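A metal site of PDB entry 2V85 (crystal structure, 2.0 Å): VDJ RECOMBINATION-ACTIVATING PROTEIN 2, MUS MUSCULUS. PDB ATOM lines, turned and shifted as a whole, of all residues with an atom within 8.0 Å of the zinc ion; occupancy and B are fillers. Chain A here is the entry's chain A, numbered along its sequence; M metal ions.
NE2 of His 50 is in hydrogen-bond range of O of Tyr 10 (2.8 Å).
SG of Cys 14 sits close to SG of Cys 15 (3.7 Å).
The side-chain sulfur (SG) of Cys 53 lies close to the backbone NH (N) of Asp 19 (3.4 Å).
SG of Cys 18 lies close to N of Val 20 (3.6 Å).
N of Cys 18 is in hydrogen-bond range of SG of Cys 15.
The zinc ion is bound by a ring nitrogen (ND1) of His 50 (2.1 Å), the side-chain sulfur (SG) of Cys 14 (2.3 Å), the side-chain sulfur (SG) of Cys 53 (2.4 Å) and the side-chain sulfur (SG) of Cys 18 (2.4 Å).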
ATOM      1  N   TYR A  10       7.849  25.601  -1.632  1.00  0.00           N
ATOM      2  CA  TYR A  10       8.838  24.538  -1.458  1.00  0.00           C
ATOM      3  C   TYR A  10      10.097  24.734  -2.293  1.00  0.00           C
ATOM      4  O   TYR A  10      11.177  24.327  -1.891  1.00  0.00           O
ATOM      5  CB  TYR A  10       8.243  23.170  -1.807  1.00  0.00           C
ATOM      6  CG  TYR A  10       7.388  22.534  -0.725  1.00  0.00           C
ATOM      7  CD1 TYR A  10       5.999  22.566  -0.800  1.00  0.00           C
ATOM      8  CD2 TYR A  10       7.980  21.888   0.360  1.00  0.00           C
ATOM      9  CE1 TYR A  10       5.211  21.952   0.183  1.00  0.00           C
ATOM     10  CE2 TYR A  10       7.204  21.272   1.340  1.00  0.00           C
ATOM     11  CZ  TYR A  10       5.826  21.309   1.246  1.00  0.00           C
ATOM     12  OH  TYR A  10       5.061  20.702   2.228  1.00  0.00           O
ATOM     13  N   TRP A  11       9.947  25.346  -3.457  1.00  0.00           N
ATOM     14  CA  TRP A  11      11.073  25.520  -4.350  1.00  0.00           C
ATOM     15  C   TRP A  11      11.716  26.902  -4.376  1.00  0.00           C
ATOM     16  O   TRP A  11      12.219  27.353  -5.388  1.00  0.00           O
ATOM     17  CB  TRP A  11      10.663  25.082  -5.759  1.00  0.00           C
ATOM     18  CG  TRP A  11      10.085  23.700  -5.746  1.00  0.00           C
ATOM     19  CD1 TRP A  11       8.799  23.351  -5.998  1.00  0.00           C
ATOM     20  CD2 TRP A  11      10.770  22.492  -5.386  1.00  0.00           C
ATOM     21  NE1 TRP A  11       8.623  21.996  -5.816  1.00  0.00           N
ATOM     22  CE2 TRP A  11       9.825  21.447  -5.443  1.00  0.00           C
ATOM     23  CE3 TRP A  11      12.087  22.192  -5.013  1.00  0.00           C
ATOM     24  CZ2 TRP A  11      10.157  20.118  -5.145  1.00  0.00           C
ATOM     25  CZ3 TRP A  11      12.419  20.875  -4.722  1.00  0.00           C
ATOM     26  CH2 TRP A  11      11.454  19.852  -4.784  1.00  0.00           C
ATOM     27  N   ILE A  12      11.699  27.556  -3.225  1.00  0.00           N
ATOM     28  CA  ILE A  12      12.296  28.869  -3.074  1.00  0.00           C
ATOM     29  C   ILE A  12      13.793  28.676  -2.819  1.00  0.00           C
ATOM     30  O   ILE A  12      14.244  27.557  -2.587  1.00  0.00           O
ATOM     31  CB  ILE A  12      11.744  29.587  -1.824  1.00  0.00           C
ATOM     32  CG1 ILE A  12      11.881  28.649  -0.619  1.00  0.00           C
ATOM     33  CG2 ILE A  12      10.298  29.985  -2.032  1.00  0.00           C
ATOM     34  CD1 ILE A  12      12.104  29.347   0.694  1.00  0.00           C
ATOM     35  N   THR A  13      14.542  29.765  -2.880  1.00  0.00           N
ATOM     36  CA  THR A  13      15.968  29.749  -2.575  1.00  0.00           C
ATOM     37  C   THR A  13      15.909  30.291  -1.151  1.00  0.00           C
ATOM     38  O   THR A  13      15.812  31.479  -0.942  1.00  0.00           O
ATOM     39  CB  THR A  13      16.770  30.685  -3.489  1.00  0.00           C
ATOM     40  OG1 THR A  13      16.767  30.162  -4.827  1.00  0.00           O
ATOM     41  CG2 THR A  13      18.207  30.808  -3.025  1.00  0.00           C
ATOM     42  N   CYS A  14      15.939  29.386  -0.164  1.00  0.00           N
ATOM     43  CA  CYS A  14      15.805  29.750   1.242  1.00  0.00           C
ATOM     44  C   CYS A  14      16.891  30.590   1.890  1.00  0.00           C
ATOM     45  O   CYS A  14      16.621  31.314   2.835  1.00  0.00           O
ATOM     46  CB  CYS A  14      15.566  28.499   2.091  1.00  0.00           C
ATOM     47  SG  CYS A  14      17.035  27.510   2.462  1.00  0.00           S
ATOM     48  N   CYS A  15      18.123  30.474   1.408  1.00  0.00           N
ATOM     49  CA  CYS A  15      19.230  31.237   1.994  1.00  0.00           C
ATOM     50  C   CYS A  15      20.365  31.353   0.985  1.00  0.00           C
ATOM     51  O   CYS A  15      20.381  30.676  -0.021  1.00  0.00           O
ATOM     52  CB  CYS A  15      19.716  30.540   3.270  1.00  0.00           C
ATOM     53  SG  CYS A  15      20.452  28.922   2.968  1.00  0.00           S
ATOM     54  N   PRO A  16      21.355  32.230   1.263  1.00  0.00           N
ATOM     55  CA  PRO A  16      22.492  32.426   0.366  1.00  0.00           C
ATOM     56  C   PRO A  16      23.198  31.148  -0.113  1.00  0.00           C
ATOM     57  O   PRO A  16      23.743  31.122  -1.189  1.00  0.00           O
ATOM     58  CB  PRO A  16      23.421  33.327   1.185  1.00  0.00           C
ATOM     59  CG  PRO A  16      22.453  34.145   1.972  1.00  0.00           C
ATOM     60  CD  PRO A  16      21.461  33.105   2.438  1.00  0.00           C
ATOM     61  N   THR A  17      23.154  30.101   0.705  1.00  0.00           N
ATOM     62  CA  THR A  17      23.822  28.852   0.333  1.00  0.00           C
ATOM     63  C   THR A  17      22.852  27.702   0.018  1.00  0.00           C
ATOM     64  O   THR A  17      23.260  26.554  -0.091  1.00  0.00           O
ATOM     65  CB  THR A  17      24.786  28.392   1.450  1.00  0.00           C
ATOM     66  OG1 THR A  17      24.043  28.137   2.650  1.00  0.00           O
ATOM     67  CG2 THR A  17      25.822  29.471   1.730  1.00  0.00           C
ATOM     68  N   CYS A  18      21.574  28.026  -0.153  1.00  0.00           N
ATOM     69  CA  CYS A  18      20.542  27.029  -0.444  1.00  0.00           C
ATOM     70  C   CYS A  18      20.932  26.018  -1.517  1.00  0.00           C
ATOM     71  O   CYS A  18      21.313  26.383  -2.615  1.00  0.00           O
ATOM     72  CB  CYS A  18      19.240  27.726  -0.849  1.00  0.00           C
ATOM     73  SG  CYS A  18      17.889  26.610  -1.266  1.00  0.00           S
ATOM     74  N   ASP A  19      20.810  24.728  -1.187  1.00  0.00           N
ATOM     75  CA  ASP A  19      21.163  23.641  -2.094  1.00  0.00           C
ATOM     76  C   ASP A  19      19.972  22.953  -2.738  1.00  0.00           C
ATOM     77  O   ASP A  19      20.145  22.083  -3.588  1.00  0.00           O
ATOM     78  CB  ASP A  19      21.964  22.580  -1.341  1.00  0.00           C
ATOM     79  CG  ASP A  19      23.442  22.871  -1.324  1.00  0.00           C
ATOM     80  OD1 ASP A  19      24.142  22.280  -0.479  1.00  0.00           O
ATOM     81  OD2 ASP A  19      23.907  23.677  -2.157  1.00  0.00           O
ATOM     82  N   VAL A  20      18.767  23.306  -2.325  1.00  0.00           N
ATOM     83  CA  VAL A  20      17.578  22.677  -2.894  1.00  0.00           C
ATOM     84  C   VAL A  20      17.159  23.316  -4.211  1.00  0.00           C
ATOM     85  O   VAL A  20      17.003  24.522  -4.303  1.00  0.00           O
ATOM     86  CB  VAL A  20      16.402  22.741  -1.885  1.00  0.00           C
ATOM     87  CG1 VAL A  20      15.112  22.271  -2.551  1.00  0.00           C
ATOM     88  CG2 VAL A  20      16.734  21.863  -0.691  1.00  0.00           C
ATOM     89  N   ASP A  21      16.999  22.469  -5.224  1.00  0.00           N
ATOM     90  CA  ASP A  21      16.620  22.911  -6.556  1.00  0.00           C
ATOM     91  C   ASP A  21      15.603  21.945  -7.136  1.00  0.00           C
ATOM     92  O   ASP A  21      15.801  20.736  -7.106  1.00  0.00           O
ATOM     93  CB  ASP A  21      17.881  22.979  -7.429  1.00  0.00           C
ATOM     94  CG  ASP A  21      17.599  23.477  -8.829  1.00  0.00           C
ATOM     95  OD1 ASP A  21      18.563  23.865  -9.513  1.00  0.00           O
ATOM     96  OD2 ASP A  21      16.422  23.457  -9.258  1.00  0.00           O
ATOM     97  N   PRO A  36      10.951  18.605  -0.189  1.00  0.00           N
ATOM     98  CA  PRO A  36      11.923  18.918   0.856  1.00  0.00           C
ATOM     99  C   PRO A  36      11.303  19.313   2.191  1.00  0.00           C
ATOM    100  O   PRO A  36      10.333  20.051   2.251  1.00  0.00           O
ATOM    101  CB  PRO A  36      12.730  20.061   0.248  1.00  0.00           C
ATOM    102  CG  PRO A  36      11.739  20.760  -0.593  1.00  0.00           C
ATOM    103  CD  PRO A  36      10.975  19.635  -1.254  1.00  0.00           C
ATOM    104  N   ALA A  37      11.867  18.774   3.264  1.00  0.00           N
ATOM    105  CA  ALA A  37      11.377  19.107   4.596  1.00  0.00           C
ATOM    106  C   ALA A  37      11.767  20.568   4.840  1.00  0.00           C
ATOM    107  O   ALA A  37      12.825  21.003   4.432  1.00  0.00           O
ATOM    108  CB  ALA A  37      12.010  18.206   5.651  1.00  0.00           C
ATOM    109  N   MET A  38      10.888  21.300   5.496  1.00  0.00           N
ATOM    110  CA  MET A  38      11.142  22.705   5.776  1.00  0.00           C
ATOM    111  C   MET A  38      10.790  23.071   7.204  1.00  0.00           C
ATOM    112  O   MET A  38       9.992  22.391   7.854  1.00  0.00           O
ATOM    113  CB  MET A  38      10.350  23.579   4.809  1.00  0.00           C
ATOM    114  CG  MET A  38      10.719  23.353   3.344  1.00  0.00           C
ATOM    115  SD  MET A  38       9.851  24.467   2.237  1.00  0.00           S
ATOM    116  CE  MET A  38      10.891  25.903   2.342  1.00  0.00           C
ATOM    117  N   TRP A  48      10.351  30.674   5.799  1.00  0.00           N
ATOM    118  CA  TRP A  48      10.599  29.242   5.655  1.00  0.00           C
ATOM    119  C   TRP A  48      11.951  28.946   5.034  1.00  0.00           C
ATOM    120  O   TRP A  48      12.373  29.610   4.091  1.00  0.00           O
ATOM    121  CB  TRP A  48       9.518  28.590   4.792  1.00  0.00           C
ATOM    122  CG  TRP A  48       8.183  28.497   5.418  1.00  0.00           C
ATOM    123  CD1 TRP A  48       7.142  29.377   5.293  1.00  0.00           C
ATOM    124  CD2 TRP A  48       7.717  27.457   6.297  1.00  0.00           C
ATOM    125  NE1 TRP A  48       6.056  28.946   6.024  1.00  0.00           N
ATOM    126  CE2 TRP A  48       6.382  27.777   6.646  1.00  0.00           C
ATOM    127  CE3 TRP A  48       8.296  26.296   6.805  1.00  0.00           C
ATOM    128  CZ2 TRP A  48       5.626  26.964   7.509  1.00  0.00           C
ATOM    129  CZ3 TRP A  48       7.547  25.489   7.663  1.00  0.00           C
ATOM    130  CH2 TRP A  48       6.227  25.830   7.994  1.00  0.00           C
ATOM    131  N   VAL A  49      12.622  27.924   5.561  1.00  0.00           N
ATOM    132  CA  VAL A  49      13.913  27.485   5.030  1.00  0.00           C
ATOM    133  C   VAL A  49      13.873  25.953   4.909  1.00  0.00           C
ATOM    134  O   VAL A  49      13.056  25.307   5.547  1.00  0.00           O
ATOM    135  CB  VAL A  49      15.102  27.868   5.953  1.00  0.00           C
ATOM    136  CG1 VAL A  49      15.285  29.383   5.982  1.00  0.00           C
ATOM    137  CG2 VAL A  49      14.880  27.316   7.348  1.00  0.00           C
ATOM    138  N   HIS A  50      14.743  25.402   4.071  1.00  0.00           N
ATOM    139  CA  HIS A  50      14.818  23.949   3.909  1.00  0.00           C
ATOM    140  C   HIS A  50      15.664  23.433   5.066  1.00  0.00           C
ATOM    141  O   HIS A  50      16.749  23.943   5.318  1.00  0.00           O
ATOM    142  CB  HIS A  50      15.481  23.568   2.586  1.00  0.00           C
ATOM    143  CG  HIS A  50      14.770  24.095   1.371  1.00  0.00           C
ATOM    144  ND1 HIS A  50      15.330  25.040   0.545  1.00  0.00           N
ATOM    145  CD2 HIS A  50      13.552  23.800   0.845  1.00  0.00           C
ATOM    146  CE1 HIS A  50      14.486  25.311  -0.441  1.00  0.00           C
ATOM    147  NE2 HIS A  50      13.404  24.569  -0.287  1.00  0.00           N
ATOM    148  N   ALA A  51      15.163  22.432   5.767  1.00  0.00           N
ATOM    149  CA  ALA A  51      15.888  21.860   6.905  1.00  0.00           C
ATOM    150  C   ALA A  51      17.302  21.443   6.532  1.00  0.00           C
ATOM    151  O   ALA A  51      18.234  21.693   7.266  1.00  0.00           O
ATOM    152  CB  ALA A  51      15.115  20.667   7.456  1.00  0.00           C
ATOM    153  N   GLN A  52      17.446  20.803   5.372  1.00  0.00           N
ATOM    154  CA  GLN A  52      18.752  20.339   4.910  1.00  0.00           C
ATOM    155  C   GLN A  52      19.755  21.474   4.713  1.00  0.00           C
ATOM    156  O   GLN A  52      20.930  21.320   4.962  1.00  0.00           O
ATOM    157  CB  GLN A  52      18.610  19.552   3.603  1.00  0.00           C
ATOM    158  CG  GLN A  52      19.851  18.744   3.249  1.00  0.00           C
ATOM    159  CD  GLN A  52      19.701  17.932   1.984  1.00  0.00           C
ATOM    160  OE1 GLN A  52      18.613  17.801   1.437  1.00  0.00           O
ATOM    161  NE2 GLN A  52      20.812  17.361   1.511  1.00  0.00           N
ATOM    162  N   CYS A  53      19.271  22.623   4.260  1.00  0.00           N
ATOM    163  CA  CYS A  53      20.145  23.758   4.029  1.00  0.00           C
ATOM    164  C   CYS A  53      20.703  24.332   5.342  1.00  0.00           C
ATOM    165  O   CYS A  53      21.682  25.068   5.328  1.00  0.00           O
ATOM    166  CB  CYS A  53      19.392  24.841   3.245  1.00  0.00           C
ATOM    167  SG  CYS A  53      18.917  24.300   1.567  1.00  0.00           S
ATOM    168  N   MET A  54      20.091  23.944   6.458  1.00  0.00           N
ATOM    169  CA  MET A  54      20.510  24.399   7.782  1.00  0.00           C
ATOM    170  C   MET A  54      21.417  23.374   8.461  1.00  0.00           C
ATOM    171  O   MET A  54      21.840  23.560   9.584  1.00  0.00           O
ATOM    172  CB  MET A  54      19.276  24.614   8.668  1.00  0.00           C
ATOM    173  CG  MET A  54      18.236  25.508   8.052  1.00  0.00           C
ATOM    174  SD  MET A  54      18.581  27.244   8.378  1.00  0.00           S
ATOM    175  CE  MET A  54      19.467  27.656   7.131  1.00  0.00           C
HETATM  176 ZN    ZN M   1      17.271  25.836   0.888  1.00  0.00          ZN
